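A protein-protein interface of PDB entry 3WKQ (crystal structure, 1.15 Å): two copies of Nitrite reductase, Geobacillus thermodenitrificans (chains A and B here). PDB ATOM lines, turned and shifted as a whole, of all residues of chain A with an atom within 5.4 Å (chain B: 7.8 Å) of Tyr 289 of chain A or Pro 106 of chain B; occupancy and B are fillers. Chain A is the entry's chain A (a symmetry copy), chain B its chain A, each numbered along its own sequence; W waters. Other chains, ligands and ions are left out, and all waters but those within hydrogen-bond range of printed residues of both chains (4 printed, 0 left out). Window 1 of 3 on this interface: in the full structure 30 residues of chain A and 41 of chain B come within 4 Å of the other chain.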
ATOM      1  N   VAL A 245      17.260   4.492   5.426  1.00  0.00           N
ATOM      2  CA  VAL A 245      16.010   5.136   5.790  1.00  0.00           C
ATOM      3  C   VAL A 245      15.548   6.011   4.638  1.00  0.00           C
ATOM      4  O   VAL A 245      16.269   6.886   4.157  1.00  0.00           O
ATOM      5  CB  VAL A 245      16.162   5.974   7.097  1.00  0.00           C
ATOM      6  CG1 VAL A 245      14.806   6.663   7.455  1.00  0.00           C
ATOM      7  CG2 VAL A 245      16.635   5.079   8.281  1.00  0.00           C
ATOM      8  N   VAL A 246      14.344   5.715   4.148  1.00  0.00           N
ATOM      9  CA  VAL A 246      13.824   6.444   2.997  1.00  0.00           C
ATOM     10  C   VAL A 246      13.533   7.886   3.362  1.00  0.00           C
ATOM     11  O   VAL A 246      12.968   8.154   4.424  1.00  0.00           O
ATOM     12  CB  VAL A 246      12.523   5.720   2.523  1.00  0.00           C
ATOM     13  CG1 VAL A 246      11.915   6.435   1.324  1.00  0.00           C
ATOM     14  CG2 VAL A 246      12.833   4.290   2.163  1.00  0.00           C
ATOM     15  N   GLY A 247      13.869   8.823   2.472  1.00  0.00           N
ATOM     16  CA  GLY A 247      13.563  10.213   2.659  1.00  0.00           C
ATOM     17  C   GLY A 247      14.560  11.002   3.472  1.00  0.00           C
ATOM     18  O   GLY A 247      14.318  12.180   3.781  1.00  0.00           O
ATOM     19  N   THR A 248      15.683  10.391   3.839  1.00  0.00           N
ATOM     20  CA  THR A 248      16.708  11.066   4.569  1.00  0.00           C
ATOM     21  C   THR A 248      18.063  10.535   4.127  1.00  0.00           C
ATOM     22  O   THR A 248      18.126   9.633   3.316  1.00  0.00           O
ATOM     23  CB  THR A 248      16.485  10.959   6.086  1.00  0.00           C
ATOM     24  OG1 THR A 248      17.375  11.842   6.775  1.00  0.00           O
ATOM     25  CG2 THR A 248      16.732   9.537   6.542  1.00  0.00           C
ATOM     26  N   VAL A 283      14.670  14.053  10.156  1.00  0.00           N
ATOM     27  CA  VAL A 283      13.387  13.925   9.463  1.00  0.00           C
ATOM     28  C   VAL A 283      12.814  15.314   9.367  1.00  0.00           C
ATOM     29  O   VAL A 283      12.501  15.988  10.321  1.00  0.00           O
ATOM     30  CB  VAL A 283      12.466  12.890  10.129  1.00  0.00           C
ATOM     31  CG1 VAL A 283      12.959  11.522   9.888  1.00  0.00           C
ATOM     32  CG2 VAL A 283      12.248  13.148  11.641  1.00  0.00           C
ATOM     33  N   THR A 284      12.741  15.820   8.118  1.00  0.00           N
ATOM     34  CA  THR A 284      12.463  17.217   7.939  1.00  0.00           C
ATOM     35  C   THR A 284      10.992  17.550   7.712  1.00  0.00           C
ATOM     36  O   THR A 284      10.655  18.723   7.799  1.00  0.00           O
ATOM     37  CB  THR A 284      13.259  17.753   6.710  1.00  0.00           C
ATOM     38  OG1 THR A 284      12.786  17.075   5.538  1.00  0.00           O
ATOM     39  CG2 THR A 284      14.752  17.607   6.874  1.00  0.00           C
ATOM     40  N   ARG A 285      10.168  16.596   7.390  1.00  0.00           N
ATOM     41  CA  ARG A 285       8.771  16.835   6.973  1.00  0.00           C
ATOM     42  C   ARG A 285       7.860  15.804   7.609  1.00  0.00           C
ATOM     43  O   ARG A 285       8.269  14.679   7.900  1.00  0.00           O
ATOM     44  CB  ARG A 285       8.649  16.732   5.431  1.00  0.00           C
ATOM     45  CG  ARG A 285       9.347  17.856   4.720  1.00  0.00           C
ATOM     46  CD  ARG A 285       9.274  17.688   3.219  1.00  0.00           C
ATOM     47  NE  ARG A 285       9.967  18.816   2.595  1.00  0.00           N
ATOM     48  CZ  ARG A 285      10.095  18.973   1.272  1.00  0.00           C
ATOM     49  NH1 ARG A 285       9.571  18.108   0.393  1.00  0.00           N
ATOM     50  NH2 ARG A 285      10.769  20.026   0.842  1.00  0.00           N
ATOM     51  N   PRO A 286       6.604  16.131   7.852  1.00  0.00           N
ATOM     52  CA  PRO A 286       5.694  15.137   8.373  1.00  0.00           C
ATOM     53  C   PRO A 286       5.451  14.063   7.358  1.00  0.00           C
ATOM     54  O   PRO A 286       5.389  14.299   6.133  1.00  0.00           O
ATOM     55  CB  PRO A 286       4.422  15.942   8.625  1.00  0.00           C
ATOM     56  CG  PRO A 286       4.500  17.095   7.644  1.00  0.00           C
ATOM     57  CD  PRO A 286       5.973  17.441   7.601  1.00  0.00           C
ATOM     58  N   GLY A 287       5.245  12.836   7.818  1.00  0.00           N
ATOM     59  CA  GLY A 287       4.907  11.716   6.955  1.00  0.00           C
ATOM     60  C   GLY A 287       5.418  10.425   7.532  1.00  0.00           C
ATOM     61  O   GLY A 287       5.924  10.418   8.669  1.00  0.00           O
ATOM     62  N   THR A 288       5.256   9.353   6.757  1.00  0.00           N
ATOM     63  CA  THR A 288       5.767   8.048   7.131  1.00  0.00           C
ATOM     64  C   THR A 288       6.993   7.709   6.323  1.00  0.00           C
ATOM     65  O   THR A 288       6.930   7.825   5.076  1.00  0.00           O
ATOM     66  CB  THR A 288       4.665   7.002   7.034  1.00  0.00           C
ATOM     67  OG1 THR A 288       3.605   7.372   7.970  1.00  0.00           O
ATOM     68  CG2 THR A 288       5.173   5.670   7.444  1.00  0.00           C
ATOM     69  N   TYR A 289       8.037   7.325   7.003  1.00  0.00           N
ATOM     70  CA  TYR A 289       9.371   7.078   6.412  1.00  0.00           C
ATOM     71  C   TYR A 289       9.667   5.597   6.544  1.00  0.00           C
ATOM     72  O   TYR A 289       9.870   5.092   7.666  1.00  0.00           O
ATOM     73  CB  TYR A 289      10.460   7.857   7.144  1.00  0.00           C
ATOM     74  CG  TYR A 289      10.370   9.337   7.011  1.00  0.00           C
ATOM     75  CD1 TYR A 289       9.293  10.078   7.521  1.00  0.00           C
ATOM     76  CD2 TYR A 289      11.409  10.049   6.379  1.00  0.00           C
ATOM     77  CE1 TYR A 289       9.269  11.452   7.362  1.00  0.00           C
ATOM     78  CE2 TYR A 289      11.401  11.418   6.257  1.00  0.00           C
ATOM     79  CZ  TYR A 289      10.301  12.139   6.777  1.00  0.00           C
ATOM     80  OH  TYR A 289      10.338  13.499   6.627  1.00  0.00           O
ATOM     81  N   PRO A 290       9.704   4.832   5.440  1.00  0.00           N
ATOM     82  CA  PRO A 290      10.111   3.417   5.551  1.00  0.00           C
ATOM     83  C   PRO A 290      11.560   3.314   5.945  1.00  0.00           C
ATOM     84  O   PRO A 290      12.409   4.135   5.563  1.00  0.00           O
ATOM     85  CB  PRO A 290       9.849   2.874   4.128  1.00  0.00           C
ATOM     86  CG  PRO A 290       8.780   3.824   3.541  1.00  0.00           C
ATOM     87  CD  PRO A 290       9.138   5.177   4.087  1.00  0.00           C
ATOM     88  N   ILE A 291      11.864   2.229   6.624  1.00  0.00           N
ATOM     89  CA  ILE A 291      13.193   1.827   7.026  1.00  0.00           C
ATOM     90  C   ILE A 291      13.408   0.438   6.441  1.00  0.00           C
ATOM     91  O   ILE A 291      12.618  -0.461   6.717  1.00  0.00           O
ATOM     92  CB  ILE A 291      13.326   1.812   8.571  1.00  0.00           C
ATOM     93  CG1 ILE A 291      13.059   3.201   9.148  1.00  0.00           C
ATOM     94  CG2 ILE A 291      14.727   1.306   8.935  1.00  0.00           C
ATOM     95  CD1 ILE A 291      12.899   3.181  10.611  1.00  0.00           C
ATOM     96  N   ALA A 305      10.405  -1.542   8.107  1.00  0.00           N
ATOM     97  CA  ALA A 305       9.785  -0.942   9.328  1.00  0.00           C
ATOM     98  C   ALA A 305       9.347   0.462   8.928  1.00  0.00           C
ATOM     99  O   ALA A 305       9.712   0.952   7.855  1.00  0.00           O
ATOM    100  CB  ALA A 305      10.770  -0.960  10.475  1.00  0.00           C
ATOM    101  N   MET A 306       8.546   1.123   9.741  1.00  0.00           N
ATOM    102  CA  MET A 306       8.047   2.463   9.419  1.00  0.00           C
ATOM    103  C   MET A 306       8.343   3.385  10.586  1.00  0.00           C
ATOM    104  O   MET A 306       8.235   3.006  11.783  1.00  0.00           O
ATOM    105  CB  MET A 306       6.519   2.399   9.211  1.00  0.00           C
ATOM    106  CG  MET A 306       6.123   1.645   8.001  1.00  0.00           C
ATOM    107  SD  MET A 306       6.709   2.304   6.410  1.00  0.00           S
ATOM    108  CE  MET A 306       6.155   1.179   5.247  1.00  0.00           C
ATOM    109  N   LEU A 307       8.673   4.655  10.251  1.00  0.00           N
ATOM    110  CA  LEU A 307       8.802   5.718  11.197  1.00  0.00           C
ATOM    111  C   LEU A 307       7.760   6.798  10.857  1.00  0.00           C
ATOM    112  O   LEU A 307       7.839   7.385   9.756  1.00  0.00           O
ATOM    113  CB  LEU A 307      10.234   6.282  11.067  1.00  0.00           C
ATOM    114  CG  LEU A 307      10.544   7.520  11.919  1.00  0.00           C
ATOM    115  CD1 LEU A 307      10.541   7.201  13.438  1.00  0.00           C
ATOM    116  CD2 LEU A 307      11.942   8.034  11.551  1.00  0.00           C
ATOM    117  N   LYS A 308       6.826   7.069  11.753  1.00  0.00           N
ATOM    118  CA  LYS A 308       5.787   8.031  11.527  1.00  0.00           C
ATOM    119  C   LYS A 308       6.178   9.313  12.224  1.00  0.00           C
ATOM    120  O   LYS A 308       6.369   9.350  13.438  1.00  0.00           O
ATOM    121  CB  LYS A 308       4.488   7.511  12.068  1.00  0.00           C
ATOM    122  CG  LYS A 308       3.359   8.473  11.859  1.00  0.00           C
ATOM    123  CD  LYS A 308       2.012   7.889  12.380  1.00  0.00           C
ATOM    124  CE  LYS A 308       0.951   8.948  12.187  1.00  0.00           C
ATOM    125  NZ  LYS A 308       0.210   8.971  10.904  1.00  0.00           N
ATOM    126  N   VAL A 309       6.288  10.393  11.443  1.00  0.00           N
ATOM    127  CA  VAL A 309       6.795  11.697  11.836  1.00  0.00           C
ATOM    128  C   VAL A 309       5.625  12.677  11.816  1.00  0.00           C
ATOM    129  O   VAL A 309       5.065  12.904  10.769  1.00  0.00           O
ATOM    130  CB  VAL A 309       7.980  12.156  10.953  1.00  0.00           C
ATOM    131  CG1 VAL A 309       8.505  13.480  11.404  1.00  0.00           C
ATOM    132  CG2 VAL A 309       9.060  11.073  10.967  1.00  0.00           C
ATOM    133  N   SER B  96       6.531   6.202  -9.505  1.00  0.00           N
ATOM    134  CA  SER B  96       6.891   7.253  -8.583  1.00  0.00           C
ATOM    135  C   SER B  96       8.423   7.452  -8.639  1.00  0.00           C
ATOM    136  O   SER B  96       9.108   6.753  -9.384  1.00  0.00           O
ATOM    137  CB  SER B  96       6.462   6.907  -7.171  1.00  0.00           C
ATOM    138  OG  SER B  96       7.044   5.669  -6.745  1.00  0.00           O
ATOM    139  N   MET B  97       8.929   8.357  -7.820  1.00  0.00           N
ATOM    140  CA  MET B  97      10.386   8.599  -7.793  1.00  0.00           C
ATOM    141  C   MET B  97      10.815   8.856  -6.371  1.00  0.00           C
ATOM    142  O   MET B  97      10.259   9.699  -5.635  1.00  0.00           O
ATOM    143  CB  MET B  97      10.729   9.865  -8.626  1.00  0.00           C
ATOM    144  CG  MET B  97      12.133  10.300  -8.489  1.00  0.00           C
ATOM    145  SD  MET B  97      13.366   9.071  -9.069  1.00  0.00           S
ATOM    146  CE  MET B  97      13.353   9.485 -10.798  1.00  0.00           C
ATOM    147  N   ASP B  98      11.867   8.121  -5.963  1.00  0.00           N
ATOM    148  CA  ASP B  98      12.582   8.277  -4.721  1.00  0.00           C
ATOM    149  C   ASP B  98      14.026   8.600  -5.078  1.00  0.00           C
ATOM    150  O   ASP B  98      14.704   7.792  -5.710  1.00  0.00           O
ATOM    151  CB  ASP B  98      12.501   6.970  -3.972  1.00  0.00           C
ATOM    152  CG  ASP B  98      13.320   6.925  -2.685  1.00  0.00           C
ATOM    153  OD1 ASP B  98      14.319   7.627  -2.541  1.00  0.00           O
ATOM    154  OD2 ASP B  98      13.015   6.041  -1.838  1.00  0.00           O
ATOM    155  N   VAL B 102      17.854  13.217  -1.431  1.00  0.00           N
ATOM    156  CA  VAL B 102      17.026  14.318  -0.902  1.00  0.00           C
ATOM    157  C   VAL B 102      16.486  14.010   0.487  1.00  0.00           C
ATOM    158  O   VAL B 102      16.310  12.851   0.882  1.00  0.00           O
ATOM    159  CB  VAL B 102      15.901  14.719  -1.861  1.00  0.00           C
ATOM    160  CG1 VAL B 102      16.464  15.090  -3.210  1.00  0.00           C
ATOM    161  CG2 VAL B 102      14.778  13.689  -1.928  1.00  0.00           C
ATOM    162  N   HIS B 103      16.171  15.091   1.188  1.00  0.00           N
ATOM    163  CA  HIS B 103      15.332  15.048   2.386  1.00  0.00           C
ATOM    164  C   HIS B 103      13.914  15.316   1.984  1.00  0.00           C
ATOM    165  O   HIS B 103      13.624  16.406   1.461  1.00  0.00           O
ATOM    166  CB  HIS B 103      15.777  16.034   3.450  1.00  0.00           C
ATOM    167  CG  HIS B 103      17.020  15.606   4.166  1.00  0.00           C
ATOM    168  ND1 HIS B 103      18.267  15.770   3.658  1.00  0.00           N
ATOM    169  CD2 HIS B 103      17.154  14.965   5.384  1.00  0.00           C
ATOM    170  CE1 HIS B 103      19.161  15.261   4.518  1.00  0.00           C
ATOM    171  NE2 HIS B 103      18.472  14.780   5.605  1.00  0.00           N
ATOM    172  N   ALA B 104      13.032  14.358   2.202  1.00  0.00           N
ATOM    173  CA  ALA B 104      11.635  14.466   1.742  1.00  0.00           C
ATOM    174  C   ALA B 104      10.759  13.643   2.627  1.00  0.00           C
ATOM    175  O   ALA B 104      11.232  12.719   3.296  1.00  0.00           O
ATOM    176  CB  ALA B 104      11.534  14.018   0.303  1.00  0.00           C
ATOM    177  N   SER B 105       9.440  13.918   2.581  1.00  0.00           N
ATOM    178  CA  SER B 105       8.475  13.065   3.248  1.00  0.00           C
ATOM    179  C   SER B 105       8.088  11.966   2.276  1.00  0.00           C
ATOM    180  O   SER B 105       7.473  12.225   1.243  1.00  0.00           O
ATOM    181  CB  SER B 105       7.220  13.863   3.535  1.00  0.00           C
ATOM    182  OG  SER B 105       6.149  12.979   3.867  1.00  0.00           O
ATOM    183  N   PRO B 106       8.397  10.659   2.519  1.00  0.00           N
ATOM    184  CA  PRO B 106       8.157   9.675   1.487  1.00  0.00           C
ATOM    185  C   PRO B 106       6.687   9.572   1.133  1.00  0.00           C
ATOM    186  O   PRO B 106       6.304   9.362  -0.010  1.00  0.00           O
ATOM    187  CB  PRO B 106       8.739   8.390   2.062  1.00  0.00           C
ATOM    188  CG  PRO B 106       9.863   8.919   2.923  1.00  0.00           C
ATOM    189  CD  PRO B 106       9.278  10.155   3.613  1.00  0.00           C
ATOM    190  N   SER B 107       5.796   9.711   2.134  1.00  0.00           N
ATOM    191  CA  SER B 107       4.347   9.528   1.979  1.00  0.00           C
ATOM    192  C   SER B 107       3.681  10.762   1.384  1.00  0.00           C
ATOM    193  O   SER B 107       2.503  10.668   1.063  1.00  0.00           O
ATOM    194  CB  SER B 107       3.749   9.143   3.313  1.00  0.00           C
ATOM    195  OG  SER B 107       4.035  10.112   4.263  1.00  0.00           O
ATOM    196  N   LYS B 108       4.391  11.849   1.171  1.00  0.00           N
ATOM    197  CA  LYS B 108       3.863  13.015   0.469  1.00  0.00           C
ATOM    198  C   LYS B 108       4.595  13.294  -0.828  1.00  0.00           C
ATOM    199  O   LYS B 108       4.004  13.750  -1.813  1.00  0.00           O
ATOM    200  CB  LYS B 108       3.895  14.272   1.383  1.00  0.00           C
ATOM    201  CG  LYS B 108       3.013  14.165   2.639  1.00  0.00           C
ATOM    202  CD  LYS B 108       3.032  15.402   3.581  1.00  0.00           C
ATOM    203  CE  LYS B 108       2.332  15.137   4.916  1.00  0.00           C
ATOM    204  NZ  LYS B 108       1.970  16.388   5.719  1.00  0.00           N
ATOM    205  N   ASP B 109       5.919  13.035  -0.864  1.00  0.00           N
ATOM    206  CA  ASP B 109       6.783  13.531  -1.926  1.00  0.00           C
ATOM    207  C   ASP B 109       7.265  12.429  -2.874  1.00  0.00           C
ATOM    208  O   ASP B 109       7.747  12.773  -3.973  1.00  0.00           O
ATOM    209  CB  ASP B 109       8.031  14.185  -1.318  1.00  0.00           C
ATOM    210  CG  ASP B 109       7.705  15.370  -0.474  1.00  0.00           C
ATOM    211  OD1 ASP B 109       6.749  16.147  -0.824  1.00  0.00           O
ATOM    212  OD2 ASP B 109       8.392  15.595   0.570  1.00  0.00           O
ATOM    213  N   PHE B 110       7.159  11.149  -2.473  1.00  0.00           N
ATOM    214  CA  PHE B 110       7.559  10.034  -3.327  1.00  0.00           C
ATOM    215  C   PHE B 110       6.313   9.213  -3.715  1.00  0.00           C
ATOM    216  O   PHE B 110       6.411   8.005  -3.893  1.00  0.00           O
ATOM    217  CB  PHE B 110       8.591   9.127  -2.624  1.00  0.00           C
ATOM    218  CG  PHE B 110       9.897   9.752  -2.209  1.00  0.00           C
ATOM    219  CD1 PHE B 110      10.372  10.953  -2.728  1.00  0.00           C
ATOM    220  CD2 PHE B 110      10.722   9.051  -1.335  1.00  0.00           C
ATOM    221  CE1 PHE B 110      11.646  11.466  -2.369  1.00  0.00           C
ATOM    222  CE2 PHE B 110      11.975   9.517  -0.991  1.00  0.00           C
ATOM    223  CZ  PHE B 110      12.462  10.690  -1.508  1.00  0.00           C
ATOM    224  N   ILE B 111       5.199   9.857  -3.877  1.00  0.00           N
ATOM    225  CA  ILE B 111       3.907   9.176  -4.095  1.00  0.00           C
ATOM    226  C   ILE B 111       3.692   8.873  -5.587  1.00  0.00           C
ATOM    227  O   ILE B 111       4.350   9.386  -6.490  1.00  0.00           O
ATOM    228  CB  ILE B 111       2.782  10.023  -3.529  1.00  0.00           C
ATOM    229  CG1 ILE B 111       2.669  11.384  -4.202  1.00  0.00           C
ATOM    230  CG2 ILE B 111       2.936  10.099  -2.025  1.00  0.00           C
ATOM    231  CD1 ILE B 111       1.376  12.131  -3.846  1.00  0.00           C
ATOM    232  N   ASP B 112       2.705   8.004  -5.799  1.00  0.00           N
ATOM    233  CA  ASP B 112       2.443   7.521  -7.143  1.00  0.00           C
ATOM    234  C   ASP B 112       1.880   8.589  -8.049  1.00  0.00           C
ATOM    235  O   ASP B 112       1.087   9.441  -7.648  1.00  0.00           O
ATOM    236  CB  ASP B 112       1.462   6.332  -7.057  1.00  0.00           C
ATOM    237  CG  ASP B 112       2.094   5.102  -6.438  1.00  0.00           C
ATOM    238  OD1 ASP B 112       3.317   5.015  -6.326  1.00  0.00           O
ATOM    239  OD2 ASP B 112       1.305   4.233  -6.048  1.00  0.00           O
ATOM    240  N   PHE B 121       7.080  17.328  -7.505  1.00  0.00           N
ATOM    241  CA  PHE B 121       7.490  17.211  -6.101  1.00  0.00           C
ATOM    242  C   PHE B 121       8.727  18.053  -5.959  1.00  0.00           C
ATOM    243  O   PHE B 121       9.557  18.091  -6.860  1.00  0.00           O
ATOM    244  CB  PHE B 121       7.775  15.716  -5.808  1.00  0.00           C
ATOM    245  CG  PHE B 121       6.662  14.837  -6.234  1.00  0.00           C
ATOM    246  CD1 PHE B 121       5.510  14.758  -5.467  1.00  0.00           C
ATOM    247  CD2 PHE B 121       6.685  14.150  -7.471  1.00  0.00           C
ATOM    248  CE1 PHE B 121       4.430  13.958  -5.854  1.00  0.00           C
ATOM    249  CE2 PHE B 121       5.592  13.351  -7.854  1.00  0.00           C
ATOM    250  CZ  PHE B 121       4.466  13.286  -7.063  1.00  0.00           C
ATOM    251  N   GLY B 136       9.462   4.211  -6.373  1.00  0.00           N
ATOM    252  CA  GLY B 136       9.054   3.857  -5.027  1.00  0.00           C
ATOM    253  C   GLY B 136       7.653   3.261  -4.919  1.00  0.00           C
ATOM    254  O   GLY B 136       7.069   3.307  -3.830  1.00  0.00           O
HETATM  255  O   HOH W   1      13.478  18.579   3.371  1.00  0.00           O
HETATM  256  O   HOH W   2      16.578  10.008   0.789  1.00  0.00           O
HETATM  257  O   HOH W   3      19.739  13.652   7.750  1.00  0.00           O
HETATM  258  O   HOH W   4      15.377   7.618   0.105  1.00  0.00           O
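Water W1 bridges OG1 of Thr 284 of chain A (2.7 Å) and O of His 103 of chain B (2.9 Å).
Water W3 bridges NE2 of His 103 of chain B and OG1 of Thr 248 of chain A.
Water W4 lies within hydrogen-bond range of the side-chain carboxylate (OD1) of Asp 98 of chain B and the backbone NH (N) of Gly 247 of chain A.
Water W2 lies within hydrogen-bond range of the backbone carbonyl oxygen of Val 102 of chain B, the backbone carbonyl oxygen of Thr 248 of chain A and the backbone NH of Gly 247 of chain A.
Val 246 of chain A touches Pro 106 of chain B.
O of Gly 247 of chain A touches CA of His 103 of chain B (3.3 Å).
Pro 106 of chain B touches Gly 247 of chain A.
O of Val 102 of chain B touches N of Thr 248 of chain A, at 3.9 Å.
Arg 285 of chain A touches Ser 105 of chain B (CB to CB, 3.7 Å).
CG of Pro 286 of chain A touches NZ of Lys 108 of chain B (3.3 Å).
Ser 105 of chain B touches Gly 287 of chain A.
Ser 107 of chain B touches Gly 287 of chain A.
Thr 288 of chain A touches Pro 106 of chain B.
CE2 of Tyr 289 of chain A touches O of Ala 104 of chain B (3.2 Å).
The side-chain hydroxyl (OG1) of Thr 248 of chain A lies within hydrogen-bond range of a ring nitrogen (NE2) of His 103 of chain B.
The backbone carbonyl oxygen (O) of Gly 247 of chain A sits at hydrogen-bond distance from the backbone NH (N) of Ala 104 of chain B, 3.0 Å away.
The backbone carbonyl oxygen (O) of Pro 286 of chain A sits at hydrogen-bond distance from the side-chain hydroxyl (OG) of Ser 105 of chain B (2.7 Å).
N of Thr 288 of chain A is in hydrogen-bond range of OG of Ser 107 of chain B, 2.9 Å away.
The side-chain carboxylate (OD2) of Asp 109 of chain B is in salt-bridge range of the guanidinium group (NH1) of Arg 285 of chain A (2.8 Å).
No position is printed for both chains.
Of the 18 printed residues of chain A, 10 touch a printed residue of chain B.
Hydrophobic or aromatic side chains of chain A within 4 Å of the printed part of chain B: Val 246, Pro 286, Tyr 289 and Pro 290.
Of the 16 printed residues of chain B, 10 touch a printed residue of chain A.
Hydrophobic or aromatic side chains of chain B within 4 Å of the printed part of chain A: His 103, Pro 106 and Phe 110.
Of the printed residues of chain B, Val 246 of chain A touches Asp 98, Pro 106 and Phe 110.
Printed residues of chain B within 4 Å of Arg 285 of chain A: Ser 105 (3.7 Å) and Asp 109 (2.8 Å).
Printed residues of chain B within 4 Å of Thr 288 of chain A: Pro 106 (3.6 Å) and Ser 107 (2.9 Å).
Tyr 289 of chain A touches just these residues of chain B: Ala 104 (3.2 Å), Ser 105 (3.9 Å) and Pro 106 (3.5 Å).
Lys 308 of chain A touches none of the printed residues of chain B.
Of the printed residues of chain A, Pro 106 of chain B touches Val 246 (3.5 Å), Gly 247 (3.9 Å), Thr 288 (3.6 Å), Tyr 289 (3.5 Å) and Pro 290 (3.8 Å).
The nearest printed residue of chain A that does not touch Pro 106 of chain B is Gly 287 of chain A (5.5 Å).
The side-chain hydroxyl of Ser 105 of chain B is in hydrogen-bond range of the backbone NH of Lys 108 of chain B, 3.4 Å away.
The backbone NH (N) of Ser 105 of chain B lies within hydrogen-bond range of the side-chain carboxylate (OD2) of Asp 109 of chain B (2.8 Å).
The backbone NH (N) of Val 246 of chain A is in hydrogen-bond range of the backbone carbonyl oxygen (O) of Pro 290 of chain A (2.9 Å).
The side-chain hydroxyl of Tyr 289 of chain A lies within hydrogen-bond range of the backbone carbonyl oxygen of Arg 285 of chain A (2.7 Å).
O of Gly 287 of chain A lies within hydrogen-bond range of N of Val 309 of chain A.
The backbone carbonyl oxygen (O) of Leu 307 of chain A is in hydrogen-bond range of the backbone NH (N) of Tyr 289 of chain A (2.8 Å).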
